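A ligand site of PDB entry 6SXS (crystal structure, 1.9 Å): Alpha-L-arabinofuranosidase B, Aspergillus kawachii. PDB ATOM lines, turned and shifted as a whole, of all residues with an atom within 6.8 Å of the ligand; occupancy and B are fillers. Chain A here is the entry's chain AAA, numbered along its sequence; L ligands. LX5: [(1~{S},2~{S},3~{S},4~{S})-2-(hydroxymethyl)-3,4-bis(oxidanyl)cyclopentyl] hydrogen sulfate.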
ATOM      1  N   PHE A  92      10.856 -30.181  -2.116  1.00  0.00           N
ATOM      2  CA  PHE A  92      11.491 -31.454  -2.512  1.00  0.00           C
ATOM      3  C   PHE A  92      12.656 -31.724  -1.579  1.00  0.00           C
ATOM      4  O   PHE A  92      13.339 -30.793  -1.129  1.00  0.00           O
ATOM      5  CB  PHE A  92      11.972 -31.446  -3.952  1.00  0.00           C
ATOM      6  CG  PHE A  92      10.836 -31.372  -4.926  1.00  0.00           C
ATOM      7  CD1 PHE A  92      10.142 -32.511  -5.283  1.00  0.00           C
ATOM      8  CD2 PHE A  92      10.486 -30.166  -5.514  1.00  0.00           C
ATOM      9  CE1 PHE A  92       9.095 -32.452  -6.201  1.00  0.00           C
ATOM     10  CE2 PHE A  92       9.453 -30.104  -6.429  1.00  0.00           C
ATOM     11  CZ  PHE A  92       8.765 -31.244  -6.779  1.00  0.00           C
ATOM     12  N   CYS A 159      14.046 -28.925 -13.695  1.00  0.00           N
ATOM     13  CA  CYS A 159      13.956 -27.744 -12.804  1.00  0.00           C
ATOM     14  C   CYS A 159      14.925 -27.927 -11.656  1.00  0.00           C
ATOM     15  O   CYS A 159      14.952 -28.992 -11.044  1.00  0.00           O
ATOM     16  CB  CYS A 159      12.542 -27.591 -12.248  1.00  0.00           C
ATOM     17  SG  CYS A 159      12.376 -26.077 -11.281  1.00  0.00           S
ATOM     18  N   CYS A 160      15.758 -26.944 -11.346  1.00  0.00           N
ATOM     19  CA  CYS A 160      15.928 -25.688 -12.059  1.00  0.00           C
ATOM     20  C   CYS A 160      17.371 -25.220 -11.752  1.00  0.00           C
ATOM     21  O   CYS A 160      17.767 -25.217 -10.570  1.00  0.00           O
ATOM     22  CB  CYS A 160      14.950 -24.591 -11.624  1.00  0.00           C
ATOM     23  SG  CYS A 160      13.327 -24.639 -12.454  1.00  0.00           S
ATOM     24  N   ASP A 162      19.247 -22.397 -11.093  1.00  0.00           N
ATOM     25  CA  ASP A 162      19.037 -20.978 -10.751  1.00  0.00           C
ATOM     26  C   ASP A 162      20.176 -20.401  -9.901  1.00  0.00           C
ATOM     27  O   ASP A 162      20.860 -21.143  -9.127  1.00  0.00           O
ATOM     28  CB  ASP A 162      17.759 -20.802  -9.930  1.00  0.00           C
ATOM     29  CG  ASP A 162      16.452 -21.044 -10.631  1.00  0.00           C
ATOM     30  OD1 ASP A 162      16.461 -21.376 -11.855  1.00  0.00           O
ATOM     31  OD2 ASP A 162      15.438 -20.903  -9.920  1.00  0.00           O
ATOM     32  N   ALA A 166      15.284 -16.078  -3.687  1.00  0.00           N
ATOM     33  CA  ALA A 166      14.229 -17.081  -3.492  1.00  0.00           C
ATOM     34  C   ALA A 166      13.608 -17.003  -2.100  1.00  0.00           C
ATOM     35  O   ALA A 166      13.784 -15.985  -1.357  1.00  0.00           O
ATOM     36  CB  ALA A 166      14.789 -18.446  -3.812  1.00  0.00           C
ATOM     37  N   GLU A 167      12.858 -18.037  -1.765  1.00  0.00           N
ATOM     38  CA  GLU A 167      12.006 -18.120  -0.564  1.00  0.00           C
ATOM     39  C   GLU A 167      12.847 -18.605   0.607  1.00  0.00           C
ATOM     40  O   GLU A 167      13.662 -19.542   0.418  1.00  0.00           O
ATOM     41  CB  GLU A 167      10.901 -19.109  -0.851  1.00  0.00           C
ATOM     42  CG  GLU A 167      10.037 -18.693  -2.022  1.00  0.00           C
ATOM     43  CD  GLU A 167      10.326 -19.441  -3.313  1.00  0.00           C
ATOM     44  OE1 GLU A 167      11.477 -19.897  -3.496  1.00  0.00           O
ATOM     45  OE2 GLU A 167       9.381 -19.593  -4.113  1.00  0.00           O
ATOM     46  N   THR A 171      10.310 -23.450   0.087  1.00  0.00           N
ATOM     47  CA  THR A 171       9.034 -23.969  -0.471  1.00  0.00           C
ATOM     48  C   THR A 171       8.470 -22.946  -1.468  1.00  0.00           C
ATOM     49  O   THR A 171       8.888 -21.743  -1.423  1.00  0.00           O
ATOM     50  CB  THR A 171       8.033 -24.281   0.662  1.00  0.00           C
ATOM     51  OG1 THR A 171       7.599 -23.047   1.216  1.00  0.00           O
ATOM     52  CG2 THR A 171       8.627 -25.108   1.781  1.00  0.00           C
ATOM     53  N   ASP A 172       7.549 -23.409  -2.314  1.00  0.00           N
ATOM     54  CA  ASP A 172       6.825 -22.557  -3.289  1.00  0.00           C
ATOM     55  C   ASP A 172       5.762 -21.752  -2.519  1.00  0.00           C
ATOM     56  O   ASP A 172       4.698 -22.310  -2.251  1.00  0.00           O
ATOM     57  CB  ASP A 172       6.212 -23.430  -4.390  1.00  0.00           C
ATOM     58  CG  ASP A 172       5.374 -22.639  -5.395  1.00  0.00           C
ATOM     59  OD1 ASP A 172       5.267 -21.393  -5.264  1.00  0.00           O
ATOM     60  OD2 ASP A 172       4.816 -23.277  -6.301  1.00  0.00           O
ATOM     61  N   MET A 178      10.172 -15.291  -6.132  1.00  0.00           N
ATOM     62  CA  MET A 178      11.530 -15.607  -6.645  1.00  0.00           C
ATOM     63  C   MET A 178      11.884 -14.547  -7.687  1.00  0.00           C
ATOM     64  O   MET A 178      10.983 -14.001  -8.319  1.00  0.00           O
ATOM     65  CB  MET A 178      11.588 -16.995  -7.312  1.00  0.00           C
ATOM     66  CG  MET A 178      11.874 -18.079  -6.331  1.00  0.00           C
ATOM     67  SD  MET A 178      11.661 -19.677  -7.007  1.00  0.00           S
ATOM     68  CE  MET A 178      13.231 -19.710  -7.867  1.00  0.00           C
ATOM     69  N   THR A 188       9.077 -26.429 -19.960  1.00  0.00           N
ATOM     70  CA  THR A 188       7.889 -26.590 -19.112  1.00  0.00           C
ATOM     71  C   THR A 188       7.143 -25.280 -18.982  1.00  0.00           C
ATOM     72  O   THR A 188       5.932 -25.330 -18.912  1.00  0.00           O
ATOM     73  CB  THR A 188       8.278 -27.101 -17.728  1.00  0.00           C
ATOM     74  OG1 THR A 188       8.845 -28.380 -18.008  1.00  0.00           O
ATOM     75  CG2 THR A 188       7.101 -27.140 -16.776  1.00  0.00           C
ATOM     76  N   TRP A 189       7.846 -24.166 -18.876  1.00  0.00           N
ATOM     77  CA  TRP A 189       7.225 -22.829 -18.741  1.00  0.00           C
ATOM     78  C   TRP A 189       7.668 -21.952 -19.932  1.00  0.00           C
ATOM     79  O   TRP A 189       7.103 -22.077 -21.005  1.00  0.00           O
ATOM     80  CB  TRP A 189       7.617 -22.225 -17.387  1.00  0.00           C
ATOM     81  CG  TRP A 189       7.273 -23.049 -16.192  1.00  0.00           C
ATOM     82  CD1 TRP A 189       6.091 -23.038 -15.500  1.00  0.00           C
ATOM     83  CD2 TRP A 189       8.170 -23.922 -15.457  1.00  0.00           C
ATOM     84  NE1 TRP A 189       6.172 -23.888 -14.426  1.00  0.00           N
ATOM     85  CE2 TRP A 189       7.425 -24.456 -14.380  1.00  0.00           C
ATOM     86  CE3 TRP A 189       9.481 -24.369 -15.651  1.00  0.00           C
ATOM     87  CZ2 TRP A 189       7.957 -25.383 -13.490  1.00  0.00           C
ATOM     88  CZ3 TRP A 189      10.021 -25.264 -14.752  1.00  0.00           C
ATOM     89  CH2 TRP A 189       9.270 -25.767 -13.680  1.00  0.00           C
ATOM     90  N   VAL A 201      14.363 -15.921 -16.409  1.00  0.00           N
ATOM     91  CA  VAL A 201      14.177 -15.439 -15.031  1.00  0.00           C
ATOM     92  C   VAL A 201      13.094 -16.311 -14.407  1.00  0.00           C
ATOM     93  O   VAL A 201      11.951 -16.356 -14.913  1.00  0.00           O
ATOM     94  CB  VAL A 201      13.875 -13.940 -14.941  1.00  0.00           C
ATOM     95  CG1 VAL A 201      13.633 -13.489 -13.497  1.00  0.00           C
ATOM     96  CG2 VAL A 201      14.993 -13.145 -15.562  1.00  0.00           C
ATOM     97  N   ASP A 202      13.486 -16.933 -13.315  1.00  0.00           N
ATOM     98  CA  ASP A 202      12.607 -17.711 -12.434  1.00  0.00           C
ATOM     99  C   ASP A 202      11.957 -16.717 -11.462  1.00  0.00           C
ATOM    100  O   ASP A 202      12.658 -16.154 -10.586  1.00  0.00           O
ATOM    101  CB  ASP A 202      13.399 -18.800 -11.700  1.00  0.00           C
ATOM    102  CG  ASP A 202      12.499 -19.862 -11.121  1.00  0.00           C
ATOM    103  OD1 ASP A 202      11.278 -19.569 -10.986  1.00  0.00           O
ATOM    104  OD2 ASP A 202      13.027 -20.982 -10.846  1.00  0.00           O
ATOM    105  N   MET A 203      10.656 -16.502 -11.655  1.00  0.00           N
ATOM    106  CA  MET A 203       9.827 -15.642 -10.771  1.00  0.00           C
ATOM    107  C   MET A 203       8.887 -16.516  -9.940  1.00  0.00           C
ATOM    108  O   MET A 203       8.063 -15.959  -9.227  1.00  0.00           O
ATOM    109  CB  MET A 203       9.028 -14.650 -11.623  1.00  0.00           C
ATOM    110  CG  MET A 203       9.941 -13.673 -12.270  1.00  0.00           C
ATOM    111  SD  MET A 203       9.077 -12.308 -13.025  1.00  0.00           S
ATOM    112  CE  MET A 203      10.230 -11.763 -14.296  1.00  0.00           C
ATOM    113  N   GLU A 204       9.079 -17.832 -10.016  1.00  0.00           N
ATOM    114  CA  GLU A 204       8.286 -18.898  -9.331  1.00  0.00           C
ATOM    115  C   GLU A 204       6.982 -19.112 -10.134  1.00  0.00           C
ATOM    116  O   GLU A 204       6.398 -18.106 -10.657  1.00  0.00           O
ATOM    117  CB  GLU A 204       8.091 -18.561  -7.857  1.00  0.00           C
ATOM    118  CG  GLU A 204       7.383 -19.672  -7.051  1.00  0.00           C
ATOM    119  CD  GLU A 204       7.996 -21.063  -7.033  1.00  0.00           C
ATOM    120  OE1 GLU A 204       8.395 -21.516  -6.008  1.00  0.00           O
ATOM    121  OE2 GLU A 204       8.094 -21.823  -8.250  1.00  0.00           O
ATOM    122  N   ASN A 205       6.582 -20.372 -10.223  1.00  0.00           N
ATOM    123  CA  ASN A 205       5.505 -20.904 -11.106  1.00  0.00           C
ATOM    124  C   ASN A 205       5.739 -20.386 -12.522  1.00  0.00           C
ATOM    125  O   ASN A 205       4.769 -20.376 -13.313  1.00  0.00           O
ATOM    126  CB  ASN A 205       4.111 -20.614 -10.567  1.00  0.00           C
ATOM    127  CG  ASN A 205       3.972 -20.986  -9.098  1.00  0.00           C
ATOM    128  OD1 ASN A 205       3.337 -20.252  -8.365  1.00  0.00           O
ATOM    129  ND2 ASN A 205       4.568 -22.090  -8.670  1.00  0.00           N
ATOM    130  N   ASN A 206       6.990 -20.151 -12.889  1.00  0.00           N
ATOM    131  CA  ASN A 206       7.338 -19.734 -14.264  1.00  0.00           C
ATOM    132  C   ASN A 206       8.839 -19.415 -14.374  1.00  0.00           C
ATOM    133  O   ASN A 206       9.377 -18.690 -13.495  1.00  0.00           O
ATOM    134  CB  ASN A 206       6.583 -18.473 -14.705  1.00  0.00           C
ATOM    135  CG  ASN A 206       5.320 -18.724 -15.493  1.00  0.00           C
ATOM    136  OD1 ASN A 206       4.317 -18.088 -15.219  1.00  0.00           O
ATOM    137  ND2 ASN A 206       5.359 -19.592 -16.482  1.00  0.00           N
ATOM    138  N   LEU A 207       9.440 -19.931 -15.430  1.00  0.00           N
ATOM    139  CA  LEU A 207      10.648 -19.355 -16.027  1.00  0.00           C
ATOM    140  C   LEU A 207      10.162 -18.464 -17.174  1.00  0.00           C
ATOM    141  O   LEU A 207       9.370 -18.963 -18.010  1.00  0.00           O
ATOM    142  CB  LEU A 207      11.508 -20.505 -16.527  1.00  0.00           C
ATOM    143  CG  LEU A 207      11.841 -21.599 -15.508  1.00  0.00           C
ATOM    144  CD1 LEU A 207      12.738 -22.653 -16.169  1.00  0.00           C
ATOM    145  CD2 LEU A 207      12.513 -21.024 -14.275  1.00  0.00           C
ATOM    146  N   TYR A 264       2.837 -11.355 -10.375  1.00  0.00           N
ATOM    147  CA  TYR A 264       4.204 -10.919 -10.753  1.00  0.00           C
ATOM    148  C   TYR A 264       4.369  -9.417 -10.622  1.00  0.00           C
ATOM    149  O   TYR A 264       5.489  -8.969 -10.828  1.00  0.00           O
ATOM    150  CB  TYR A 264       4.593 -11.488 -12.106  1.00  0.00           C
ATOM    151  CG  TYR A 264       4.593 -12.993 -12.124  1.00  0.00           C
ATOM    152  CD1 TYR A 264       5.538 -13.720 -11.415  1.00  0.00           C
ATOM    153  CD2 TYR A 264       3.601 -13.690 -12.795  1.00  0.00           C
ATOM    154  CE1 TYR A 264       5.517 -15.113 -11.432  1.00  0.00           C
ATOM    155  CE2 TYR A 264       3.570 -15.077 -12.804  1.00  0.00           C
ATOM    156  CZ  TYR A 264       4.539 -15.790 -12.126  1.00  0.00           C
ATOM    157  OH  TYR A 264       4.508 -17.147 -12.170  1.00  0.00           O
ATOM    158  N   ILE A 274      19.693 -18.835  -3.620  1.00  0.00           N
ATOM    159  CA  ILE A 274      19.818 -20.223  -4.110  1.00  0.00           C
ATOM    160  C   ILE A 274      20.898 -20.274  -5.209  1.00  0.00           C
ATOM    161  O   ILE A 274      21.038 -19.290  -5.999  1.00  0.00           O
ATOM    162  CB  ILE A 274      18.491 -20.789  -4.657  1.00  0.00           C
ATOM    163  CG1 ILE A 274      17.892 -19.875  -5.712  1.00  0.00           C
ATOM    164  CG2 ILE A 274      17.519 -21.092  -3.533  1.00  0.00           C
ATOM    165  CD1 ILE A 274      16.601 -20.408  -6.349  1.00  0.00           C
ATOM    166  N   ILE A 277      19.478 -24.883  -7.919  1.00  0.00           N
ATOM    167  CA  ILE A 277      18.206 -25.525  -7.482  1.00  0.00           C
ATOM    168  C   ILE A 277      17.061 -24.529  -7.716  1.00  0.00           C
ATOM    169  O   ILE A 277      17.316 -23.302  -7.821  1.00  0.00           O
ATOM    170  CB  ILE A 277      18.266 -25.961  -5.997  1.00  0.00           C
ATOM    171  CG1 ILE A 277      18.649 -24.806  -5.074  1.00  0.00           C
ATOM    172  CG2 ILE A 277      19.197 -27.163  -5.817  1.00  0.00           C
ATOM    173  CD1 ILE A 277      18.366 -25.058  -3.621  1.00  0.00           C
ATOM    174  N   GLY A 278      15.847 -25.032  -7.773  1.00  0.00           N
ATOM    175  CA  GLY A 278      14.631 -24.177  -7.708  1.00  0.00           C
ATOM    176  C   GLY A 278      14.382 -23.654  -6.302  1.00  0.00           C
ATOM    177  O   GLY A 278      15.018 -24.178  -5.356  1.00  0.00           O
ATOM    178  N   GLY A 279      13.478 -22.674  -6.153  1.00  0.00           N
ATOM    179  CA  GLY A 279      13.104 -22.067  -4.846  1.00  0.00           C
ATOM    180  C   GLY A 279      12.544 -23.119  -3.896  1.00  0.00           C
ATOM    181  O   GLY A 279      12.789 -23.017  -2.663  1.00  0.00           O
ATOM    182  N   ASP A 280      11.818 -24.086  -4.443  1.00  0.00           N
ATOM    183  CA  ASP A 280      11.151 -25.185  -3.681  1.00  0.00           C
ATOM    184  C   ASP A 280      12.093 -26.376  -3.496  1.00  0.00           C
ATOM    185  O   ASP A 280      11.616 -27.475  -3.153  1.00  0.00           O
ATOM    186  CB  ASP A 280       9.848 -25.582  -4.360  1.00  0.00           C
ATOM    187  CG  ASP A 280      10.017 -26.161  -5.746  1.00  0.00           C
ATOM    188  OD1 ASP A 280      11.168 -26.348  -6.212  1.00  0.00           O
ATOM    189  OD2 ASP A 280       8.973 -26.457  -6.340  1.00  0.00           O
ATOM    190  N   ASN A 281      13.379 -26.169  -3.728  1.00  0.00           N
ATOM    191  CA  ASN A 281      14.451 -27.192  -3.732  1.00  0.00           C
ATOM    192  C   ASN A 281      14.285 -28.206  -4.866  1.00  0.00           C
ATOM    193  O   ASN A 281      14.844 -29.321  -4.742  1.00  0.00           O
ATOM    194  CB  ASN A 281      14.609 -27.934  -2.402  1.00  0.00           C
ATOM    195  CG  ASN A 281      15.950 -28.636  -2.336  1.00  0.00           C
ATOM    196  OD1 ASN A 281      16.937 -28.031  -2.768  1.00  0.00           O
ATOM    197  ND2 ASN A 281      15.975 -29.865  -1.788  1.00  0.00           N
ATOM    198  N   SER A 282      13.625 -27.877  -5.976  1.00  0.00           N
ATOM    199  CA  SER A 282      13.688 -28.717  -7.198  1.00  0.00           C
ATOM    200  C   SER A 282      15.170 -28.964  -7.471  1.00  0.00           C
ATOM    201  O   SER A 282      15.912 -27.967  -7.522  1.00  0.00           O
ATOM    202  CB  SER A 282      13.012 -28.079  -8.359  1.00  0.00           C
ATOM    203  OG  SER A 282      11.636 -27.879  -8.097  1.00  0.00           O
HETATM  204  C1  LX5 L   1       8.484 -23.547  -9.733  1.00  0.00           C
HETATM  205  C2  LX5 L   1       8.616 -23.162  -8.270  1.00  0.00           C
HETATM  206  C6  LX5 L   1       9.755 -22.491 -11.640  1.00  0.00           C
HETATM  207  C5  LX5 L   1       9.888 -23.321 -10.361  1.00  0.00           C
HETATM  208  C3  LX5 L   1      10.130 -23.323  -7.973  1.00  0.00           C
HETATM  209  C4  LX5 L   1      10.735 -22.682  -9.211  1.00  0.00           C
HETATM  210  O7  LX5 L   1       9.331 -21.142 -11.377  1.00  0.00           O
HETATM  211  O8  LX5 L   1      12.104 -22.954  -9.295  1.00  0.00           O
HETATM  212  O9  LX5 L   1      10.650 -22.750  -6.749  1.00  0.00           O
HETATM  213  O10 LX5 L   1       7.971 -24.861  -9.916  1.00  0.00           O
HETATM  214  S11 LX5 L   1       6.439 -25.080  -9.965  1.00  0.00           S
HETATM  215  O12 LX5 L   1       5.851 -24.680  -8.712  1.00  0.00           O
HETATM  216  O13 LX5 L   1       5.939 -24.184 -11.024  1.00  0.00           O
HETATM  217  O14 LX5 L   1       6.343 -26.452 -10.317  1.00  0.00           O
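The side-chain amide nitrogen (ND2) of Asn 205 lies within hydrogen-bond range of the side-chain carboxylate (OD2) of Asp 172, at 2.7 Å. The side-chain sulfur (SD) of Met 178 sits close to the backbone NH (N) of Gly 279 (3.6 Å). OD2 of Asp 202 lies close to OD2 of Asp 162 (2.6 Å). The side-chain sulfur (SG) of Cys 159 sits close to the side-chain hydroxyl (OG) of Ser 282 (3.7 Å). The side-chain hydroxyl (OH) of Tyr 264 is in hydrogen-bond range of the backbone carbonyl oxygen (O) of Asn 205, 3.4 Å away. The backbone carbonyl oxygen (O) of Asp 280 lies within hydrogen-bond range of the backbone NH (N) of Phe 92 (3.0 Å). The backbone NH (N) of Gly 278 sits at hydrogen-bond distance from the backbone carbonyl oxygen (O) of Cys 160 (3.4 Å). The side-chain sulfur of Cys 159 forms a disulfide with the side-chain sulfur of Cys 160 (2.1 Å).
The side-chain carboxylate (OE2) of Glu 204 is bonded to a carbon (C2) of the ligand (1.4 Å). The side-chain carboxylate (OD1) of Asp 202 sits at hydrogen-bond distance from an oxygen (O7) of the ligand (2.5 Å). The backbone NH of Asn 206 sits at hydrogen-bond distance from an oxygen (O7) of the ligand (3.0 Å). An oxygen (O7) of the ligand sits at hydrogen-bond distance from the backbone carbonyl oxygen of Asn 206 (3.2 Å). ND2 of Asn 205 lies within hydrogen-bond range of O12 of the ligand (2.9 Å). The side-chain sulfur (SG) of Cys 160 sits at hydrogen-bond distance from an oxygen (O8) of the ligand (3.8 Å). O12 of the ligand sits close to OD2 of Asp 172 (3.0 Å). An oxygen (O13) of the ligand sits close to the indole nitrogen of Trp 189. N of Asn 205 is in hydrogen-bond range of O7 of the ligand (3.1 Å). The side-chain sulfur (SD) of Met 178 sits at hydrogen-bond distance from an oxygen (O9) of the ligand (3.2 Å). N of Gly 279 is in hydrogen-bond range of O9 of the ligand. The backbone NH (N) of Asp 280 lies within hydrogen-bond range of an oxygen (O9) of the ligand (2.9 Å). The side-chain sulfur (SG) of Cys 159 is in hydrogen-bond range of an oxygen (O8) of the ligand.
Asp 162 touches the ligand. Gly 278 touches the ligand (CA to O8, 3.2 Å). 13 residues have an atom within 4 Å of the ligand: Cys 159, Cys 160, Asp 162, Asp 172, Met 178, Trp 189, Asp 202, Glu 204, Asn 205, Asn 206, Gly 278, Gly 279 and Asp 280. The nearest printed residue that does not touch the ligand is Leu 207 (4.1 Å).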
